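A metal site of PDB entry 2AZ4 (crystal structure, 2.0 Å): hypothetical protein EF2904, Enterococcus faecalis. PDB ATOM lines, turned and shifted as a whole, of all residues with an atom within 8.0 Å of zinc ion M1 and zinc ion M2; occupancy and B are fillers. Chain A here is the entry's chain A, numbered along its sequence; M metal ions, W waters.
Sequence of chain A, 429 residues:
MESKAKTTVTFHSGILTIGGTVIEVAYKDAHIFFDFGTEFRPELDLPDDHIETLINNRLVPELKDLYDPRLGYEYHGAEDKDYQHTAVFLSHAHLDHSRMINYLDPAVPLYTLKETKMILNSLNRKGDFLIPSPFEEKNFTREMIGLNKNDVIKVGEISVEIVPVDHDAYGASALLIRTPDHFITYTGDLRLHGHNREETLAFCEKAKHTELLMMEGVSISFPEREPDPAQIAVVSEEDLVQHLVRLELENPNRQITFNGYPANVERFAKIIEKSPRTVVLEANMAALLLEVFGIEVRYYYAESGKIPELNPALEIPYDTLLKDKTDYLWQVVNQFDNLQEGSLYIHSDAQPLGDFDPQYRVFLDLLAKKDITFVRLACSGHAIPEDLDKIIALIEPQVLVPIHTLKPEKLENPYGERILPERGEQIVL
ND1 of His 97 is in hydrogen-bond range of OD2 of Asp 35, at 2.8 Å. The side-chain carboxylate (OD1) of Asp 168 lies close to a ring nitrogen (ND1) of His 167. O of Gly 381 lies within hydrogen-bond range of ND1 of His 167. The backbone NH (N) of Val 218 is in hydrogen-bond range of the backbone carbonyl oxygen (O) of His 404 (3.4 Å). A ring nitrogen (ND1) of His 404 lies close to the backbone NH (N) of Gly 19 (3.5 Å). A ring nitrogen (ND1) of His 92 is in hydrogen-bond range of the side-chain hydroxyl of Ser 91, at 2.6 Å. The backbone NH of Gly 20 sits at hydrogen-bond distance from the backbone carbonyl oxygen of Asp 96 (2.9 Å).
Zinc ion M1 is bound by water W3 (2.2 Å). Zinc ion M1 is bound by NE2 of His 167 (2.2 Å). Zinc ion M1 is bound by a ring nitrogen (NE2) of His 92. A ring nitrogen (ND1) of His 94 binds zinc ion M1 (2.3 Å). Zinc ion M1 is bound by water W1, 2.3 Å away. Zinc ion M1 is bound by OD2 of Asp 189 (2.4 Å). Zinc ion M1 has six donor atoms within binding distance.
Four residues have an atom within 4 Å of zinc ion M1: His 92, His 94, His 167 and Asp 189. The nearest printed residue that does not touch zinc ion M1 is His 97 (4.1 Å).
Four residues have an atom within 4 Å of zinc ion M2: Asp 96, His 97, Asp 189 and His 404. Along chain A the residues within 4 Å of zinc ion M2 span positions 96 to 404. The nearest printed residue that does not touch zinc ion M2 is His 382 (4.2 Å).
Zinc ion M2 is bound by NE2 of His 97 (2.2 Å), OD2 of Asp 189 (2.2 Å), NE2 of His 404 (2.3 Å), OD2 of Asp 96 (2.3 Å), water W1 (2.3 Å) and water W2 (2.3 Å). Zinc ion M2 has six donor atoms within binding distance.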
ATOM      1  N   ILE A  18      -8.074  21.045  29.938  1.00  0.00           N
ATOM      2  CA  ILE A  18      -6.667  21.033  29.563  1.00  0.00           C
ATOM      3  C   ILE A  18      -5.848  21.011  30.838  1.00  0.00           C
ATOM      4  O   ILE A  18      -5.487  22.055  31.379  1.00  0.00           O
ATOM      5  CB  ILE A  18      -6.346  22.213  28.617  1.00  0.00           C
ATOM      6  CG1 ILE A  18      -7.267  22.107  27.387  1.00  0.00           C
ATOM      7  CG2 ILE A  18      -4.863  22.185  28.242  1.00  0.00           C
ATOM      8  CD1 ILE A  18      -6.895  22.971  26.194  1.00  0.00           C
ATOM      9  N   GLY A  19      -5.628  19.811  31.364  1.00  0.00           N
ATOM     10  CA  GLY A  19      -4.859  19.636  32.583  1.00  0.00           C
ATOM     11  C   GLY A  19      -5.386  18.513  33.432  1.00  0.00           C
ATOM     12  O   GLY A  19      -6.595  18.300  33.519  1.00  0.00           O
ATOM     13  N   GLY A  20      -4.473  17.789  34.062  1.00  0.00           N
ATOM     14  CA  GLY A  20      -4.864  16.755  35.009  1.00  0.00           C
ATOM     15  C   GLY A  20      -5.152  15.408  34.379  1.00  0.00           C
ATOM     16  O   GLY A  20      -5.858  14.602  34.982  1.00  0.00           O
ATOM     17  N   THR A  21      -4.585  15.157  33.190  1.00  0.00           N
ATOM     18  CA  THR A  21      -4.610  13.813  32.601  1.00  0.00           C
ATOM     19  C   THR A  21      -3.994  12.784  33.525  1.00  0.00           C
ATOM     20  O   THR A  21      -2.818  12.889  33.904  1.00  0.00           O
ATOM     21  CB  THR A  21      -3.892  13.722  31.245  1.00  0.00           C
ATOM     22  OG1 THR A  21      -4.493  14.626  30.326  1.00  0.00           O
ATOM     23  CG2 THR A  21      -4.016  12.336  30.641  1.00  0.00           C
ATOM     24  N   ASP A  35      -0.315  11.305  33.348  1.00  0.00           N
ATOM     25  CA  ASP A  35       0.756  11.909  34.138  1.00  0.00           C
ATOM     26  C   ASP A  35       0.252  12.030  35.586  1.00  0.00           C
ATOM     27  O   ASP A  35      -0.350  11.074  36.100  1.00  0.00           O
ATOM     28  CB  ASP A  35       1.135  13.276  33.525  1.00  0.00           C
ATOM     29  CG  ASP A  35       1.815  13.122  32.162  1.00  0.00           C
ATOM     30  OD1 ASP A  35       2.662  12.211  32.029  1.00  0.00           O
ATOM     31  OD2 ASP A  35       1.543  13.923  31.236  1.00  0.00           O
ATOM     32  N   SER A  91       5.375  12.961  31.627  1.00  0.00           N
ATOM     33  CA  SER A  91       5.739  13.346  30.277  1.00  0.00           C
ATOM     34  C   SER A  91       6.677  14.555  30.281  1.00  0.00           C
ATOM     35  O   SER A  91       7.651  14.568  29.555  1.00  0.00           O
ATOM     36  CB  SER A  91       4.482  13.616  29.392  1.00  0.00           C
ATOM     37  OG  SER A  91       3.846  14.865  29.659  1.00  0.00           O
ATOM     38  N   HIS A  92       6.353  15.554  31.096  1.00  0.00           N
ATOM     39  CA  HIS A  92       7.143  16.777  31.214  1.00  0.00           C
ATOM     40  C   HIS A  92       6.773  17.577  32.471  1.00  0.00           C
ATOM     41  O   HIS A  92       5.813  17.246  33.189  1.00  0.00           O
ATOM     42  CB  HIS A  92       7.068  17.640  29.933  1.00  0.00           C
ATOM     43  CG  HIS A  92       5.704  18.190  29.634  1.00  0.00           C
ATOM     44  ND1 HIS A  92       4.598  17.380  29.439  1.00  0.00           N
ATOM     45  CD2 HIS A  92       5.263  19.459  29.486  1.00  0.00           C
ATOM     46  CE1 HIS A  92       3.546  18.139  29.149  1.00  0.00           C
ATOM     47  NE2 HIS A  92       3.924  19.402  29.193  1.00  0.00           N
ATOM     48  N   ALA A  93       7.517  18.656  32.723  1.00  0.00           N
ATOM     49  CA  ALA A  93       7.437  19.425  33.972  1.00  0.00           C
ATOM     50  C   ALA A  93       6.213  20.335  34.176  1.00  0.00           C
ATOM     51  O   ALA A  93       5.882  20.705  35.325  1.00  0.00           O
ATOM     52  CB  ALA A  93       8.726  20.212  34.171  1.00  0.00           C
ATOM     53  N   HIS A  94       5.553  20.705  33.084  1.00  0.00           N
ATOM     54  CA  HIS A  94       4.443  21.660  33.176  1.00  0.00           C
ATOM     55  C   HIS A  94       3.457  21.315  34.269  1.00  0.00           C
ATOM     56  O   HIS A  94       3.189  20.145  34.543  1.00  0.00           O
ATOM     57  CB  HIS A  94       3.759  21.852  31.792  1.00  0.00           C
ATOM     58  CG  HIS A  94       4.564  22.698  30.864  1.00  0.00           C
ATOM     59  ND1 HIS A  94       4.364  22.697  29.495  1.00  0.00           N
ATOM     60  CD2 HIS A  94       5.552  23.589  31.088  1.00  0.00           C
ATOM     61  CE1 HIS A  94       5.216  23.537  28.922  1.00  0.00           C
ATOM     62  NE2 HIS A  94       5.947  24.093  29.868  1.00  0.00           N
ATOM     63  N   LEU A  95       2.929  22.359  34.912  1.00  0.00           N
ATOM     64  CA  LEU A  95       2.077  22.220  36.106  1.00  0.00           C
ATOM     65  C   LEU A  95       0.880  21.257  35.939  1.00  0.00           C
ATOM     66  O   LEU A  95       0.553  20.473  36.854  1.00  0.00           O
ATOM     67  CB  LEU A  95       1.565  23.621  36.495  1.00  0.00           C
ATOM     68  CG  LEU A  95       0.894  23.834  37.854  1.00  0.00           C
ATOM     69  CD1 LEU A  95       1.862  23.533  39.023  1.00  0.00           C
ATOM     70  CD2 LEU A  95       0.319  25.262  37.953  1.00  0.00           C
ATOM     71  N   ASP A  96       0.252  21.337  34.748  1.00  0.00           N
ATOM     72  CA  ASP A  96      -0.954  20.570  34.425  1.00  0.00           C
ATOM     73  C   ASP A  96      -0.660  19.084  34.198  1.00  0.00           C
ATOM     74  O   ASP A  96      -1.586  18.285  34.021  1.00  0.00           O
ATOM     75  CB  ASP A  96      -1.718  21.193  33.232  1.00  0.00           C
ATOM     76  CG  ASP A  96      -0.868  21.333  31.960  1.00  0.00           C
ATOM     77  OD1 ASP A  96       0.283  21.840  32.047  1.00  0.00           O
ATOM     78  OD2 ASP A  96      -1.349  20.931  30.862  1.00  0.00           O
ATOM     79  N   HIS A  97       0.630  18.734  34.255  1.00  0.00           N
ATOM     80  CA  HIS A  97       1.115  17.355  34.231  1.00  0.00           C
ATOM     81  C   HIS A  97       1.814  16.905  35.513  1.00  0.00           C
ATOM     82  O   HIS A  97       1.939  15.712  35.753  1.00  0.00           O
ATOM     83  CB  HIS A  97       2.035  17.145  33.014  1.00  0.00           C
ATOM     84  CG  HIS A  97       1.384  17.541  31.724  1.00  0.00           C
ATOM     85  ND1 HIS A  97       0.805  16.621  30.863  1.00  0.00           N
ATOM     86  CD2 HIS A  97       1.116  18.755  31.199  1.00  0.00           C
ATOM     87  CE1 HIS A  97       0.239  17.256  29.862  1.00  0.00           C
ATOM     88  NE2 HIS A  97       0.429  18.556  30.018  1.00  0.00           N
ATOM     89  N   HIS A 167       8.615  20.026  22.489  1.00  0.00           N
ATOM     90  CA  HIS A 167       7.599  20.796  23.244  1.00  0.00           C
ATOM     91  C   HIS A 167       8.348  22.009  23.855  1.00  0.00           C
ATOM     92  O   HIS A 167       9.564  22.037  23.878  1.00  0.00           O
ATOM     93  CB  HIS A 167       6.915  19.898  24.297  1.00  0.00           C
ATOM     94  CG  HIS A 167       5.780  20.547  25.036  1.00  0.00           C
ATOM     95  ND1 HIS A 167       4.779  21.261  24.406  1.00  0.00           N
ATOM     96  CD2 HIS A 167       5.458  20.545  26.353  1.00  0.00           C
ATOM     97  CE1 HIS A 167       3.924  21.714  25.312  1.00  0.00           C
ATOM     98  NE2 HIS A 167       4.304  21.286  26.497  1.00  0.00           N
ATOM     99  N   ASP A 168       7.626  23.021  24.316  1.00  0.00           N
ATOM    100  CA  ASP A 168       8.290  24.185  24.896  1.00  0.00           C
ATOM    101  C   ASP A 168       8.796  23.930  26.324  1.00  0.00           C
ATOM    102  O   ASP A 168       9.405  24.827  26.899  1.00  0.00           O
ATOM    103  CB  ASP A 168       7.416  25.459  24.798  1.00  0.00           C
ATOM    104  CG  ASP A 168       6.093  25.325  25.514  1.00  0.00           C
ATOM    105  OD1 ASP A 168       5.720  24.186  25.820  1.00  0.00           O
ATOM    106  OD2 ASP A 168       5.407  26.352  25.787  1.00  0.00           O
ATOM    107  N   ALA A 169       8.508  22.762  26.909  1.00  0.00           N
ATOM    108  CA  ALA A 169       9.205  22.306  28.120  1.00  0.00           C
ATOM    109  C   ALA A 169      10.351  21.434  27.659  1.00  0.00           C
ATOM    110  O   ALA A 169      10.121  20.428  26.966  1.00  0.00           O
ATOM    111  CB  ALA A 169       8.298  21.493  29.056  1.00  0.00           C
ATOM    112  N   ALA A 172      10.734  17.094  27.475  1.00  0.00           N
ATOM    113  CA  ALA A 172       9.389  16.571  27.232  1.00  0.00           C
ATOM    114  C   ALA A 172       9.476  15.245  26.497  1.00  0.00           C
ATOM    115  O   ALA A 172      10.356  15.060  25.643  1.00  0.00           O
ATOM    116  CB  ALA A 172       8.558  17.555  26.412  1.00  0.00           C
ATOM    117  N   TYR A 186       1.092   7.271  24.227  1.00  0.00           N
ATOM    118  CA  TYR A 186       0.640   8.479  24.874  1.00  0.00           C
ATOM    119  C   TYR A 186       1.560   9.599  24.399  1.00  0.00           C
ATOM    120  O   TYR A 186       2.760   9.520  24.619  1.00  0.00           O
ATOM    121  CB  TYR A 186       0.762   8.317  26.382  1.00  0.00           C
ATOM    122  CG  TYR A 186       0.498   9.585  27.154  1.00  0.00           C
ATOM    123  CD1 TYR A 186      -0.705  10.299  26.993  1.00  0.00           C
ATOM    124  CD2 TYR A 186       1.474  10.117  28.010  1.00  0.00           C
ATOM    125  CE1 TYR A 186      -0.945  11.479  27.724  1.00  0.00           C
ATOM    126  CE2 TYR A 186       1.249  11.290  28.725  1.00  0.00           C
ATOM    127  CZ  TYR A 186       0.039  11.968  28.586  1.00  0.00           C
ATOM    128  OH  TYR A 186      -0.190  13.114  29.291  1.00  0.00           O
ATOM    129  N   GLY A 188       1.876  12.777  25.233  1.00  0.00           N
ATOM    130  CA  GLY A 188       2.165  13.912  26.108  1.00  0.00           C
ATOM    131  C   GLY A 188       1.753  15.156  25.332  1.00  0.00           C
ATOM    132  O   GLY A 188       0.835  15.089  24.487  1.00  0.00           O
ATOM    133  N   ASP A 189       2.420  16.261  25.617  1.00  0.00           N
ATOM    134  CA  ASP A 189       2.285  17.481  24.824  1.00  0.00           C
ATOM    135  C   ASP A 189       3.407  17.541  23.813  1.00  0.00           C
ATOM    136  O   ASP A 189       4.538  17.159  24.138  1.00  0.00           O
ATOM    137  CB  ASP A 189       2.419  18.694  25.745  1.00  0.00           C
ATOM    138  CG  ASP A 189       1.217  18.929  26.602  1.00  0.00           C
ATOM    139  OD1 ASP A 189       0.229  18.159  26.554  1.00  0.00           O
ATOM    140  OD2 ASP A 189       1.256  19.919  27.337  1.00  0.00           O
ATOM    141  N   LEU A 190       3.120  18.045  22.602  1.00  0.00           N
ATOM    142  CA  LEU A 190       4.097  18.063  21.504  1.00  0.00           C
ATOM    143  C   LEU A 190       3.771  18.958  20.317  1.00  0.00           C
ATOM    144  O   LEU A 190       2.646  19.387  20.122  1.00  0.00           O
ATOM    145  CB  LEU A 190       4.405  16.665  20.960  1.00  0.00           C
ATOM    146  CG  LEU A 190       3.424  15.521  20.661  1.00  0.00           C
ATOM    147  CD1 LEU A 190       1.944  15.840  20.477  1.00  0.00           C
ATOM    148  CD2 LEU A 190       3.943  14.643  19.565  1.00  0.00           C
ATOM    149  N   GLU A 216      -2.922  14.560  22.573  1.00  0.00           N
ATOM    150  CA  GLU A 216      -3.368  15.898  22.897  1.00  0.00           C
ATOM    151  C   GLU A 216      -4.061  16.618  21.733  1.00  0.00           C
ATOM    152  O   GLU A 216      -3.819  16.306  20.548  1.00  0.00           O
ATOM    153  CB  GLU A 216      -2.187  16.760  23.397  1.00  0.00           C
ATOM    154  CG  GLU A 216      -1.156  17.033  22.320  1.00  0.00           C
ATOM    155  CD  GLU A 216      -0.834  18.510  22.202  1.00  0.00           C
ATOM    156  OE1 GLU A 216       0.295  18.899  22.567  1.00  0.00           O
ATOM    157  OE2 GLU A 216      -1.690  19.290  21.718  1.00  0.00           O
ATOM    158  N   VAL A 218      -4.708  20.358  22.094  1.00  0.00           N
ATOM    159  CA  VAL A 218      -4.754  21.675  22.713  1.00  0.00           C
ATOM    160  C   VAL A 218      -5.085  22.786  21.688  1.00  0.00           C
ATOM    161  O   VAL A 218      -6.038  23.550  21.890  1.00  0.00           O
ATOM    162  CB  VAL A 218      -3.462  21.994  23.496  1.00  0.00           C
ATOM    163  CG1 VAL A 218      -3.478  23.414  24.022  1.00  0.00           C
ATOM    164  CG2 VAL A 218      -3.294  20.987  24.639  1.00  0.00           C
ATOM    165  N   GLY A 381       3.912  26.019  22.542  1.00  0.00           N
ATOM    166  CA  GLY A 381       4.473  24.705  22.729  1.00  0.00           C
ATOM    167  C   GLY A 381       3.697  23.566  22.056  1.00  0.00           C
ATOM    168  O   GLY A 381       4.180  22.440  22.016  1.00  0.00           O
ATOM    169  N   HIS A 382       2.492  23.857  21.538  1.00  0.00           N
ATOM    170  CA  HIS A 382       1.570  22.815  21.021  1.00  0.00           C
ATOM    171  C   HIS A 382       1.488  22.772  19.510  1.00  0.00           C
ATOM    172  O   HIS A 382       1.645  23.803  18.840  1.00  0.00           O
ATOM    173  CB  HIS A 382       0.167  22.984  21.616  1.00  0.00           C
ATOM    174  CG  HIS A 382       0.125  22.774  23.092  1.00  0.00           C
ATOM    175  ND1 HIS A 382       0.089  21.521  23.669  1.00  0.00           N
ATOM    176  CD2 HIS A 382       0.150  23.661  24.119  1.00  0.00           C
ATOM    177  CE1 HIS A 382       0.090  21.651  24.987  1.00  0.00           C
ATOM    178  NE2 HIS A 382       0.102  22.931  25.288  1.00  0.00           N
ATOM    179  N   HIS A 404      -6.685  15.828  26.447  1.00  0.00           N
ATOM    180  CA  HIS A 404      -6.067  17.135  26.652  1.00  0.00           C
ATOM    181  C   HIS A 404      -6.612  18.106  25.590  1.00  0.00           C
ATOM    182  O   HIS A 404      -5.848  18.717  24.827  1.00  0.00           O
ATOM    183  CB  HIS A 404      -4.530  16.975  26.572  1.00  0.00           C
ATOM    184  CG  HIS A 404      -3.764  17.911  27.456  1.00  0.00           C
ATOM    185  ND1 HIS A 404      -4.070  18.099  28.788  1.00  0.00           N
ATOM    186  CD2 HIS A 404      -2.665  18.670  27.204  1.00  0.00           C
ATOM    187  CE1 HIS A 404      -3.201  18.949  29.309  1.00  0.00           C
ATOM    188  NE2 HIS A 404      -2.338  19.307  28.372  1.00  0.00           N
HETATM  189 ZN    ZN M   1       2.983  21.283  28.286  1.00  0.00          ZN
HETATM  190 ZN    ZN M   2      -0.321  20.249  28.903  1.00  0.00          ZN
HETATM  191  O   HOH W   1       1.274  21.702  29.794  1.00  0.00           O
HETATM  192  O   HOH W   2      -0.879  22.274  27.874  1.00  0.00           O
HETATM  193  O   HOH W   3       1.745  22.988  27.660  1.00  0.00           O
